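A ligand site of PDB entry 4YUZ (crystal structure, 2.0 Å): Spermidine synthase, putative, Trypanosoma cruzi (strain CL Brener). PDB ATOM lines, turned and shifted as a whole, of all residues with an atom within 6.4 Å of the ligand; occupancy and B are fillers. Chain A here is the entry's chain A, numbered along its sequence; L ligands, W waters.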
ATOM      1  N   PHE A  47       6.356 -15.462 -36.070  1.00  0.00           N
ATOM      2  CA  PHE A  47       6.889 -14.590 -35.035  1.00  0.00           C
ATOM      3  C   PHE A  47       8.130 -13.782 -35.398  1.00  0.00           C
ATOM      4  O   PHE A  47       8.372 -12.812 -34.728  1.00  0.00           O
ATOM      5  CB  PHE A  47       7.220 -15.419 -33.797  1.00  0.00           C
ATOM      6  CG  PHE A  47       6.028 -16.143 -33.253  1.00  0.00           C
ATOM      7  CD1 PHE A  47       5.119 -15.451 -32.435  1.00  0.00           C
ATOM      8  CD2 PHE A  47       5.755 -17.428 -33.643  1.00  0.00           C
ATOM      9  CE1 PHE A  47       3.972 -16.078 -31.967  1.00  0.00           C
ATOM     10  CE2 PHE A  47       4.591 -18.067 -33.180  1.00  0.00           C
ATOM     11  CZ  PHE A  47       3.723 -17.383 -32.310  1.00  0.00           C
ATOM     12  N   GLN A  48       8.905 -14.178 -36.409  1.00  0.00           N
ATOM     13  CA  GLN A  48      10.191 -13.477 -36.668  1.00  0.00           C
ATOM     14  C   GLN A  48      10.731 -13.884 -38.023  1.00  0.00           C
ATOM     15  O   GLN A  48      10.232 -14.826 -38.601  1.00  0.00           O
ATOM     16  CB  GLN A  48      11.205 -13.794 -35.567  1.00  0.00           C
ATOM     17  CG  GLN A  48      11.467 -15.296 -35.463  1.00  0.00           C
ATOM     18  CD  GLN A  48      11.995 -15.760 -34.110  1.00  0.00           C
ATOM     19  OE1 GLN A  48      12.682 -15.032 -33.399  1.00  0.00           O
ATOM     20  NE2 GLN A  48      11.695 -17.005 -33.770  1.00  0.00           N
ATOM     21  N   MET A  65      22.594 -19.357 -38.949  1.00  0.00           N
ATOM     22  CA  MET A  65      21.216 -19.052 -38.726  1.00  0.00           C
ATOM     23  C   MET A  65      21.084 -17.650 -38.122  1.00  0.00           C
ATOM     24  O   MET A  65      21.751 -17.300 -37.129  1.00  0.00           O
ATOM     25  CB  MET A  65      20.481 -20.083 -37.829  1.00  0.00           C
ATOM     26  CG  MET A  65      19.217 -19.432 -37.203  1.00  0.00           C
ATOM     27  SD  MET A  65      18.198 -20.522 -36.204  1.00  0.00           S
ATOM     28  CE  MET A  65      18.483 -22.056 -37.051  1.00  0.00           C
ATOM     29  N   LEU A  67      18.028 -14.584 -36.982  1.00  0.00           N
ATOM     30  CA  LEU A  67      16.645 -14.320 -36.644  1.00  0.00           C
ATOM     31  C   LEU A  67      16.478 -12.810 -36.618  1.00  0.00           C
ATOM     32  O   LEU A  67      17.277 -12.123 -35.942  1.00  0.00           O
ATOM     33  CB  LEU A  67      16.199 -14.913 -35.261  1.00  0.00           C
ATOM     34  CG  LEU A  67      16.311 -16.421 -34.996  1.00  0.00           C
ATOM     35  CD1 LEU A  67      15.790 -16.744 -33.594  1.00  0.00           C
ATOM     36  CD2 LEU A  67      15.604 -17.253 -36.036  1.00  0.00           C
ATOM     37  N   GLN A  72      22.416 -15.919 -34.830  1.00  0.00           N
ATOM     38  CA  GLN A  72      22.061 -16.594 -33.570  1.00  0.00           C
ATOM     39  C   GLN A  72      22.945 -17.826 -33.396  1.00  0.00           C
ATOM     40  O   GLN A  72      23.280 -18.177 -32.285  1.00  0.00           O
ATOM     41  CB  GLN A  72      20.617 -17.131 -33.591  1.00  0.00           C
ATOM     42  CG  GLN A  72      19.529 -16.112 -33.730  1.00  0.00           C
ATOM     43  CD  GLN A  72      19.345 -15.222 -32.527  1.00  0.00           C
ATOM     44  OE1 GLN A  72      18.997 -15.696 -31.434  1.00  0.00           O
ATOM     45  NE2 GLN A  72      19.514 -13.920 -32.712  1.00  0.00           N
ATOM     46  N   VAL A  73      23.286 -18.499 -34.508  1.00  0.00           N
ATOM     47  CA  VAL A  73      23.988 -19.786 -34.414  1.00  0.00           C
ATOM     48  C   VAL A  73      24.903 -19.877 -35.599  1.00  0.00           C
ATOM     49  O   VAL A  73      24.483 -19.456 -36.708  1.00  0.00           O
ATOM     50  CB  VAL A  73      23.014 -20.990 -34.418  1.00  0.00           C
ATOM     51  CG1 VAL A  73      23.804 -22.296 -34.461  1.00  0.00           C
ATOM     52  CG2 VAL A  73      22.168 -20.970 -33.129  1.00  0.00           C
ATOM     53  N   TYR A  81      28.539 -20.466 -26.594  1.00  0.00           N
ATOM     54  CA  TYR A  81      27.327 -19.947 -25.912  1.00  0.00           C
ATOM     55  C   TYR A  81      26.549 -21.148 -25.314  1.00  0.00           C
ATOM     56  O   TYR A  81      26.017 -21.062 -24.221  1.00  0.00           O
ATOM     57  CB  TYR A  81      26.395 -19.112 -26.834  1.00  0.00           C
ATOM     58  CG  TYR A  81      26.525 -19.293 -28.301  1.00  0.00           C
ATOM     59  CD1 TYR A  81      27.745 -18.919 -28.998  1.00  0.00           C
ATOM     60  CD2 TYR A  81      25.426 -19.808 -29.081  1.00  0.00           C
ATOM     61  CE1 TYR A  81      27.820 -19.041 -30.376  1.00  0.00           C
ATOM     62  CE2 TYR A  81      25.529 -19.920 -30.482  1.00  0.00           C
ATOM     63  CZ  TYR A  81      26.717 -19.528 -31.132  1.00  0.00           C
ATOM     64  OH  TYR A  81      26.879 -19.623 -32.550  1.00  0.00           O
ATOM     65  N   HIS A  82      26.495 -22.291 -26.025  1.00  0.00           N
ATOM     66  CA  HIS A  82      25.713 -23.439 -25.450  1.00  0.00           C
ATOM     67  C   HIS A  82      26.342 -24.055 -24.209  1.00  0.00           C
ATOM     68  O   HIS A  82      25.649 -24.382 -23.218  1.00  0.00           O
ATOM     69  CB  HIS A  82      25.456 -24.449 -26.556  1.00  0.00           C
ATOM     70  CG  HIS A  82      24.561 -23.847 -27.620  1.00  0.00           C
ATOM     71  ND1 HIS A  82      24.691 -24.127 -28.965  1.00  0.00           N
ATOM     72  CD2 HIS A  82      23.650 -22.874 -27.533  1.00  0.00           C
ATOM     73  CE1 HIS A  82      23.815 -23.394 -29.647  1.00  0.00           C
ATOM     74  NE2 HIS A  82      23.167 -22.624 -28.795  1.00  0.00           N
ATOM     75  N   ILE A 102      13.708 -21.830 -21.755  1.00  0.00           N
ATOM     76  CA  ILE A 102      12.859 -20.959 -22.511  1.00  0.00           C
ATOM     77  C   ILE A 102      13.636 -20.434 -23.699  1.00  0.00           C
ATOM     78  O   ILE A 102      14.749 -19.886 -23.518  1.00  0.00           O
ATOM     79  CB  ILE A 102      12.390 -19.774 -21.633  1.00  0.00           C
ATOM     80  CG1 ILE A 102      11.511 -20.353 -20.508  1.00  0.00           C
ATOM     81  CG2 ILE A 102      11.572 -18.826 -22.505  1.00  0.00           C
ATOM     82  CD1 ILE A 102      11.168 -19.366 -19.393  1.00  0.00           C
ATOM     83  N   GLY A 103      13.077 -20.674 -24.872  1.00  0.00           N
ATOM     84  CA  GLY A 103      13.749 -20.450 -26.122  1.00  0.00           C
ATOM     85  C   GLY A 103      14.493 -21.719 -26.502  1.00  0.00           C
ATOM     86  O   GLY A 103      13.981 -22.826 -26.276  1.00  0.00           O
ATOM     87  N   GLY A 104      15.669 -21.536 -27.108  1.00  0.00           N
ATOM     88  CA  GLY A 104      16.593 -22.660 -27.369  1.00  0.00           C
ATOM     89  C   GLY A 104      16.088 -23.719 -28.338  1.00  0.00           C
ATOM     90  O   GLY A 104      16.433 -24.893 -28.227  1.00  0.00           O
ATOM     91  N   GLY A 105      15.297 -23.260 -29.320  1.00  0.00           N
ATOM     92  CA  GLY A 105      14.631 -24.152 -30.243  1.00  0.00           C
ATOM     93  C   GLY A 105      15.624 -24.862 -31.157  1.00  0.00           C
ATOM     94  O   GLY A 105      15.295 -25.920 -31.702  1.00  0.00           O
ATOM     95  N   ASP A 106      16.809 -24.292 -31.336  1.00  0.00           N
ATOM     96  CA  ASP A 106      17.948 -24.993 -32.015  1.00  0.00           C
ATOM     97  C   ASP A 106      18.465 -26.267 -31.335  1.00  0.00           C
ATOM     98  O   ASP A 106      18.999 -27.140 -32.002  1.00  0.00           O
ATOM     99  CB  ASP A 106      19.079 -23.988 -32.257  1.00  0.00           C
ATOM    100  CG  ASP A 106      19.563 -23.354 -30.980  1.00  0.00           C
ATOM    101  OD1 ASP A 106      20.336 -24.031 -30.301  1.00  0.00           O
ATOM    102  OD2 ASP A 106      19.183 -22.178 -30.637  1.00  0.00           O
ATOM    103  N   GLY A 107      18.299 -26.431 -30.027  1.00  0.00           N
ATOM    104  CA  GLY A 107      18.757 -27.661 -29.414  1.00  0.00           C
ATOM    105  C   GLY A 107      20.091 -27.585 -28.645  1.00  0.00           C
ATOM    106  O   GLY A 107      20.389 -28.494 -27.902  1.00  0.00           O
ATOM    107  N   GLY A 108      20.859 -26.503 -28.792  1.00  0.00           N
ATOM    108  CA  GLY A 108      22.226 -26.482 -28.256  1.00  0.00           C
ATOM    109  C   GLY A 108      22.320 -26.481 -26.737  1.00  0.00           C
ATOM    110  O   GLY A 108      23.104 -27.243 -26.146  1.00  0.00           O
ATOM    111  N   VAL A 109      21.561 -25.597 -26.079  1.00  0.00           N
ATOM    112  CA  VAL A 109      21.567 -25.644 -24.610  1.00  0.00           C
ATOM    113  C   VAL A 109      21.123 -26.975 -24.110  1.00  0.00           C
ATOM    114  O   VAL A 109      21.656 -27.511 -23.132  1.00  0.00           O
ATOM    115  CB  VAL A 109      20.676 -24.542 -24.004  1.00  0.00           C
ATOM    116  CG1 VAL A 109      20.700 -24.613 -22.493  1.00  0.00           C
ATOM    117  CG2 VAL A 109      21.256 -23.178 -24.406  1.00  0.00           C
ATOM    118  N   VAL A 125      10.669 -24.894 -24.063  1.00  0.00           N
ATOM    119  CA  VAL A 125       9.540 -24.153 -24.614  1.00  0.00           C
ATOM    120  C   VAL A 125      10.029 -22.979 -25.479  1.00  0.00           C
ATOM    121  O   VAL A 125      10.528 -21.927 -24.942  1.00  0.00           O
ATOM    122  CB  VAL A 125       8.633 -23.566 -23.453  1.00  0.00           C
ATOM    123  CG1 VAL A 125       7.432 -22.823 -24.015  1.00  0.00           C
ATOM    124  CG2 VAL A 125       8.156 -24.698 -22.488  1.00  0.00           C
ATOM    125  N   ASP A 126       9.815 -23.116 -26.789  1.00  0.00           N
ATOM    126  CA  ASP A 126      10.214 -22.142 -27.773  1.00  0.00           C
ATOM    127  C   ASP A 126       8.959 -21.728 -28.600  1.00  0.00           C
ATOM    128  O   ASP A 126       8.239 -22.585 -29.132  1.00  0.00           O
ATOM    129  CB  ASP A 126      11.322 -22.713 -28.755  1.00  0.00           C
ATOM    130  CG  ASP A 126      11.946 -21.591 -29.627  1.00  0.00           C
ATOM    131  OD1 ASP A 126      11.190 -20.860 -30.376  1.00  0.00           O
ATOM    132  OD2 ASP A 126      13.188 -21.342 -29.484  1.00  0.00           O
ATOM    133  N   ILE A 127       8.768 -20.423 -28.757  1.00  0.00           N
ATOM    134  CA  ILE A 127       7.570 -19.844 -29.355  1.00  0.00           C
ATOM    135  C   ILE A 127       7.428 -20.189 -30.797  1.00  0.00           C
ATOM    136  O   ILE A 127       6.303 -20.238 -31.318  1.00  0.00           O
ATOM    137  CB  ILE A 127       7.526 -18.308 -29.157  1.00  0.00           C
ATOM    138  CG1 ILE A 127       6.094 -17.755 -29.407  1.00  0.00           C
ATOM    139  CG2 ILE A 127       8.541 -17.607 -30.061  1.00  0.00           C
ATOM    140  CD1 ILE A 127       5.929 -16.373 -28.820  1.00  0.00           C
ATOM    141  N   ASP A 128       8.548 -20.472 -31.455  1.00  0.00           N
ATOM    142  CA  ASP A 128       8.598 -20.662 -32.850  1.00  0.00           C
ATOM    143  C   ASP A 128       8.927 -22.079 -33.304  1.00  0.00           C
ATOM    144  O   ASP A 128      10.077 -22.453 -33.371  1.00  0.00           O
ATOM    145  CB  ASP A 128       9.565 -19.631 -33.443  1.00  0.00           C
ATOM    146  CG  ASP A 128       9.333 -19.394 -34.984  1.00  0.00           C
ATOM    147  OD1 ASP A 128       8.722 -20.231 -35.665  1.00  0.00           O
ATOM    148  OD2 ASP A 128       9.817 -18.379 -35.501  1.00  0.00           O
ATOM    149  N   VAL A 131      11.604 -22.594 -36.177  1.00  0.00           N
ATOM    150  CA  VAL A 131      13.009 -22.686 -35.715  1.00  0.00           C
ATOM    151  C   VAL A 131      13.440 -24.155 -35.486  1.00  0.00           C
ATOM    152  O   VAL A 131      14.514 -24.577 -35.993  1.00  0.00           O
ATOM    153  CB  VAL A 131      13.266 -21.814 -34.466  1.00  0.00           C
ATOM    154  CG1 VAL A 131      14.655 -22.090 -33.882  1.00  0.00           C
ATOM    155  CG2 VAL A 131      13.067 -20.301 -34.774  1.00  0.00           C
ATOM    156  N   GLY A 156       5.501 -22.770 -28.021  1.00  0.00           N
ATOM    157  CA  GLY A 156       4.639 -21.913 -27.217  1.00  0.00           C
ATOM    158  C   GLY A 156       5.411 -20.785 -26.574  1.00  0.00           C
ATOM    159  O   GLY A 156       6.657 -20.775 -26.562  1.00  0.00           O
ATOM    160  N   ASP A 157       4.660 -19.814 -26.058  1.00  0.00           N
ATOM    161  CA  ASP A 157       5.219 -18.577 -25.527  1.00  0.00           C
ATOM    162  C   ASP A 157       5.669 -18.881 -24.144  1.00  0.00           C
ATOM    163  O   ASP A 157       4.882 -19.298 -23.342  1.00  0.00           O
ATOM    164  CB  ASP A 157       4.144 -17.485 -25.467  1.00  0.00           C
ATOM    165  CG  ASP A 157       4.699 -16.077 -25.092  1.00  0.00           C
ATOM    166  OD1 ASP A 157       5.832 -15.905 -24.597  1.00  0.00           O
ATOM    167  OD2 ASP A 157       3.988 -15.087 -25.234  1.00  0.00           O
ATOM    168  N   GLY A 158       6.926 -18.572 -23.828  1.00  0.00           N
ATOM    169  CA  GLY A 158       7.468 -18.847 -22.508  1.00  0.00           C
ATOM    170  C   GLY A 158       6.834 -18.004 -21.457  1.00  0.00           C
ATOM    171  O   GLY A 158       6.781 -18.391 -20.293  1.00  0.00           O
ATOM    172  N   LEU A 159       6.379 -16.811 -21.848  1.00  0.00           N
ATOM    173  CA  LEU A 159       5.621 -15.966 -20.915  1.00  0.00           C
ATOM    174  C   LEU A 159       4.347 -16.677 -20.392  1.00  0.00           C
ATOM    175  O   LEU A 159       4.105 -16.743 -19.195  1.00  0.00           O
ATOM    176  CB  LEU A 159       5.299 -14.628 -21.587  1.00  0.00           C
ATOM    177  CG  LEU A 159       4.526 -13.548 -20.812  1.00  0.00           C
ATOM    178  CD1 LEU A 159       5.047 -13.270 -19.406  1.00  0.00           C
ATOM    179  CD2 LEU A 159       4.482 -12.265 -21.621  1.00  0.00           C
ATOM    180  N   ASP A 176      17.233 -18.643 -23.018  1.00  0.00           N
ATOM    181  CA  ASP A 176      18.043 -18.580 -24.203  1.00  0.00           C
ATOM    182  C   ASP A 176      17.233 -17.909 -25.311  1.00  0.00           C
ATOM    183  O   ASP A 176      16.802 -18.570 -26.282  1.00  0.00           O
ATOM    184  CB  ASP A 176      18.351 -20.018 -24.601  1.00  0.00           C
ATOM    185  CG  ASP A 176      19.183 -20.104 -25.871  1.00  0.00           C
ATOM    186  OD1 ASP A 176      19.898 -19.149 -26.155  1.00  0.00           O
ATOM    187  OD2 ASP A 176      19.118 -21.140 -26.559  1.00  0.00           O
ATOM    188  N   THR A 177      16.925 -16.625 -25.152  1.00  0.00           N
ATOM    189  CA  THR A 177      15.986 -16.028 -26.123  1.00  0.00           C
ATOM    190  C   THR A 177      16.638 -14.919 -26.955  1.00  0.00           C
ATOM    191  O   THR A 177      17.695 -14.389 -26.574  1.00  0.00           O
ATOM    192  CB  THR A 177      14.676 -15.502 -25.475  1.00  0.00           C
ATOM    193  OG1 THR A 177      15.022 -14.642 -24.399  1.00  0.00           O
ATOM    194  CG2 THR A 177      13.809 -16.604 -24.934  1.00  0.00           C
ATOM    195  N   THR A 178      15.957 -14.539 -28.036  1.00  0.00           N
ATOM    196  CA  THR A 178      16.487 -13.674 -29.110  1.00  0.00           C
ATOM    197  C   THR A 178      17.056 -12.316 -28.676  1.00  0.00           C
ATOM    198  O   THR A 178      16.410 -11.555 -27.958  1.00  0.00           O
ATOM    199  CB  THR A 178      15.427 -13.461 -30.198  1.00  0.00           C
ATOM    200  OG1 THR A 178      14.115 -13.617 -29.621  1.00  0.00           O
ATOM    201  CG2 THR A 178      15.591 -14.492 -31.283  1.00  0.00           C
HETATM  202  C1  LIG L   1      21.536 -19.595 -29.603  1.00  0.00           C
HETATM  203  N1  LIG L   1      20.927 -20.853 -29.103  1.00  0.00           N
HETATM  204  C2  LIG L   1      20.562 -18.536 -29.125  1.00  0.00           C
HETATM  205  C3  LIG L   1      19.333 -18.243 -29.954  1.00  0.00           C
HETATM  206  S1  LIG L   1      17.759 -19.200 -29.788  1.00  0.00           S
HETATM  207  C4  LIG L   1      17.661 -19.422 -31.609  1.00  0.00           C
HETATM  208  C5  LIG L   1      16.528 -17.858 -29.493  1.00  0.00           C
HETATM  209  C6  LIG L   1      15.078 -18.484 -29.442  1.00  0.00           C
HETATM  210  O1  LIG L   1      14.171 -17.808 -28.567  1.00  0.00           O
HETATM  211  C7  LIG L   1      12.868 -18.145 -29.082  1.00  0.00           C
HETATM  212  C8  LIG L   1      13.023 -17.814 -30.552  1.00  0.00           C
HETATM  213  O2  LIG L   1      12.027 -18.363 -31.392  1.00  0.00           O
HETATM  214  C9  LIG L   1      14.397 -18.389 -30.811  1.00  0.00           C
HETATM  215  O3  LIG L   1      14.469 -19.728 -31.339  1.00  0.00           O
HETATM  216  N2  LIG L   1      11.923 -17.291 -28.427  1.00  0.00           N
HETATM  217  C10 LIG L   1      11.761 -15.955 -28.670  1.00  0.00           C
HETATM  218  N3  LIG L   1      10.810 -15.447 -27.922  1.00  0.00           N
HETATM  219  C11 LIG L   1      10.339 -16.495 -27.148  1.00  0.00           C
HETATM  220  C12 LIG L   1       9.318 -16.548 -26.178  1.00  0.00           C
HETATM  221  N4  LIG L   1       8.558 -15.398 -25.814  1.00  0.00           N
HETATM  222  C13 LIG L   1      11.016 -17.651 -27.452  1.00  0.00           C
HETATM  223  N5  LIG L   1      10.779 -18.835 -26.919  1.00  0.00           N
HETATM  224  C14 LIG L   1       9.832 -18.774 -25.985  1.00  0.00           C
HETATM  225  N6  LIG L   1       9.089 -17.721 -25.575  1.00  0.00           N
HETATM  226  O   HOH W   1      19.872 -23.504 -27.383  1.00  0.00           O
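Water W1 lies within hydrogen-bond range of the side-chain carboxylate of Asp 176 (2.6 Å), the backbone NH of Val 109 (3.0 Å), the side-chain carboxylate of Asp 106 (3.0 Å), a nitrogen (N1) of the ligand (3.3 Å) and the backbone NH of Gly 108 (3.5 Å).
N1 of the ligand lies within salt-bridge range of OD2 of Asp 106.
NE2 of Gln 48 is in hydrogen-bond range of O2 of the ligand, 2.8 Å away.
The backbone NH of Gly 158 sits at hydrogen-bond distance from a nitrogen (N6) of the ligand, at 2.9 Å.
O3 of the ligand is in hydrogen-bond range of OD2 of Asp 126.
The side-chain carboxylate (OD2) of Asp 176 is in salt-bridge range of a nitrogen (N1) of the ligand, at 3.1 Å.
N of Ile 127 lies within hydrogen-bond range of N5 of the ligand, at 3.2 Å.
O of Asp 176 sits close to S1 of the ligand (3.7 Å).
NE2 of His 82 sits at hydrogen-bond distance from N1 of the ligand, 2.9 Å away.
The side-chain carboxylate (OD1) of Asp 157 lies within hydrogen-bond range of a nitrogen (N4) of the ligand, at 3.0 Å.
Merely in contact with the ligand: Leu 67 (3.5 Å), Gln 72 (3.0 Å), Val 73 (3.8 Å), Tyr 81 (3.9 Å), Ile 102 (3.9 Å), Gly 103 (3.5 Å), Gly 104 (3.9 Å), Val 125 (3.4 Å), Asp 128 (3.4 Å), Val 131 (3.5 Å), Gly 156 (3.8 Å), Thr 177 (3.5 Å) and Thr 178 (3.5 Å).
Hydrophobic or aromatic side chains within 4 Å of the ligand: Leu 67, Val 73, Tyr 81, His 82, Ile 102, Ile 127 and Val 131.
Within 4 Å of the ligand: Gln 48, Leu 67, Gln 72, Val 73, Tyr 81, His 82, Ile 102, Gly 103, Gly 104, Asp 106, Val 125, Asp 126, Ile 127, Asp 128, Val 131, Gly 156, Asp 157, Gly 158, Asp 176, Thr 177 and Thr 178.
The nearest printed residue that does not touch the ligand is Gly 105 (4.2 Å).
The side-chain amide nitrogen (NE2) of Gln 48 lies within hydrogen-bond range of the side-chain carboxylate (OD2) of Asp 128, 2.9 Å away.
The side-chain carboxylate of Asp 157 lies within hydrogen-bond range of the backbone NH of Leu 159.
N of Met 65 is in hydrogen-bond range of O of Val 73.
The backbone carbonyl oxygen (O) of Asp 176 sits at hydrogen-bond distance from the backbone NH (N) of Gly 104.
The side-chain carboxylate of Asp 126 lies within hydrogen-bond range of the backbone NH of Gly 105 (2.9 Å).
O of Gly 156 is in hydrogen-bond range of N of Ile 127, 3.1 Å away.
The backbone carbonyl oxygen (O) of Val 125 is in hydrogen-bond range of the backbone NH (N) of Gly 103.
The backbone NH (N) of Asp 176 sits at hydrogen-bond distance from the backbone carbonyl oxygen (O) of Ile 102.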
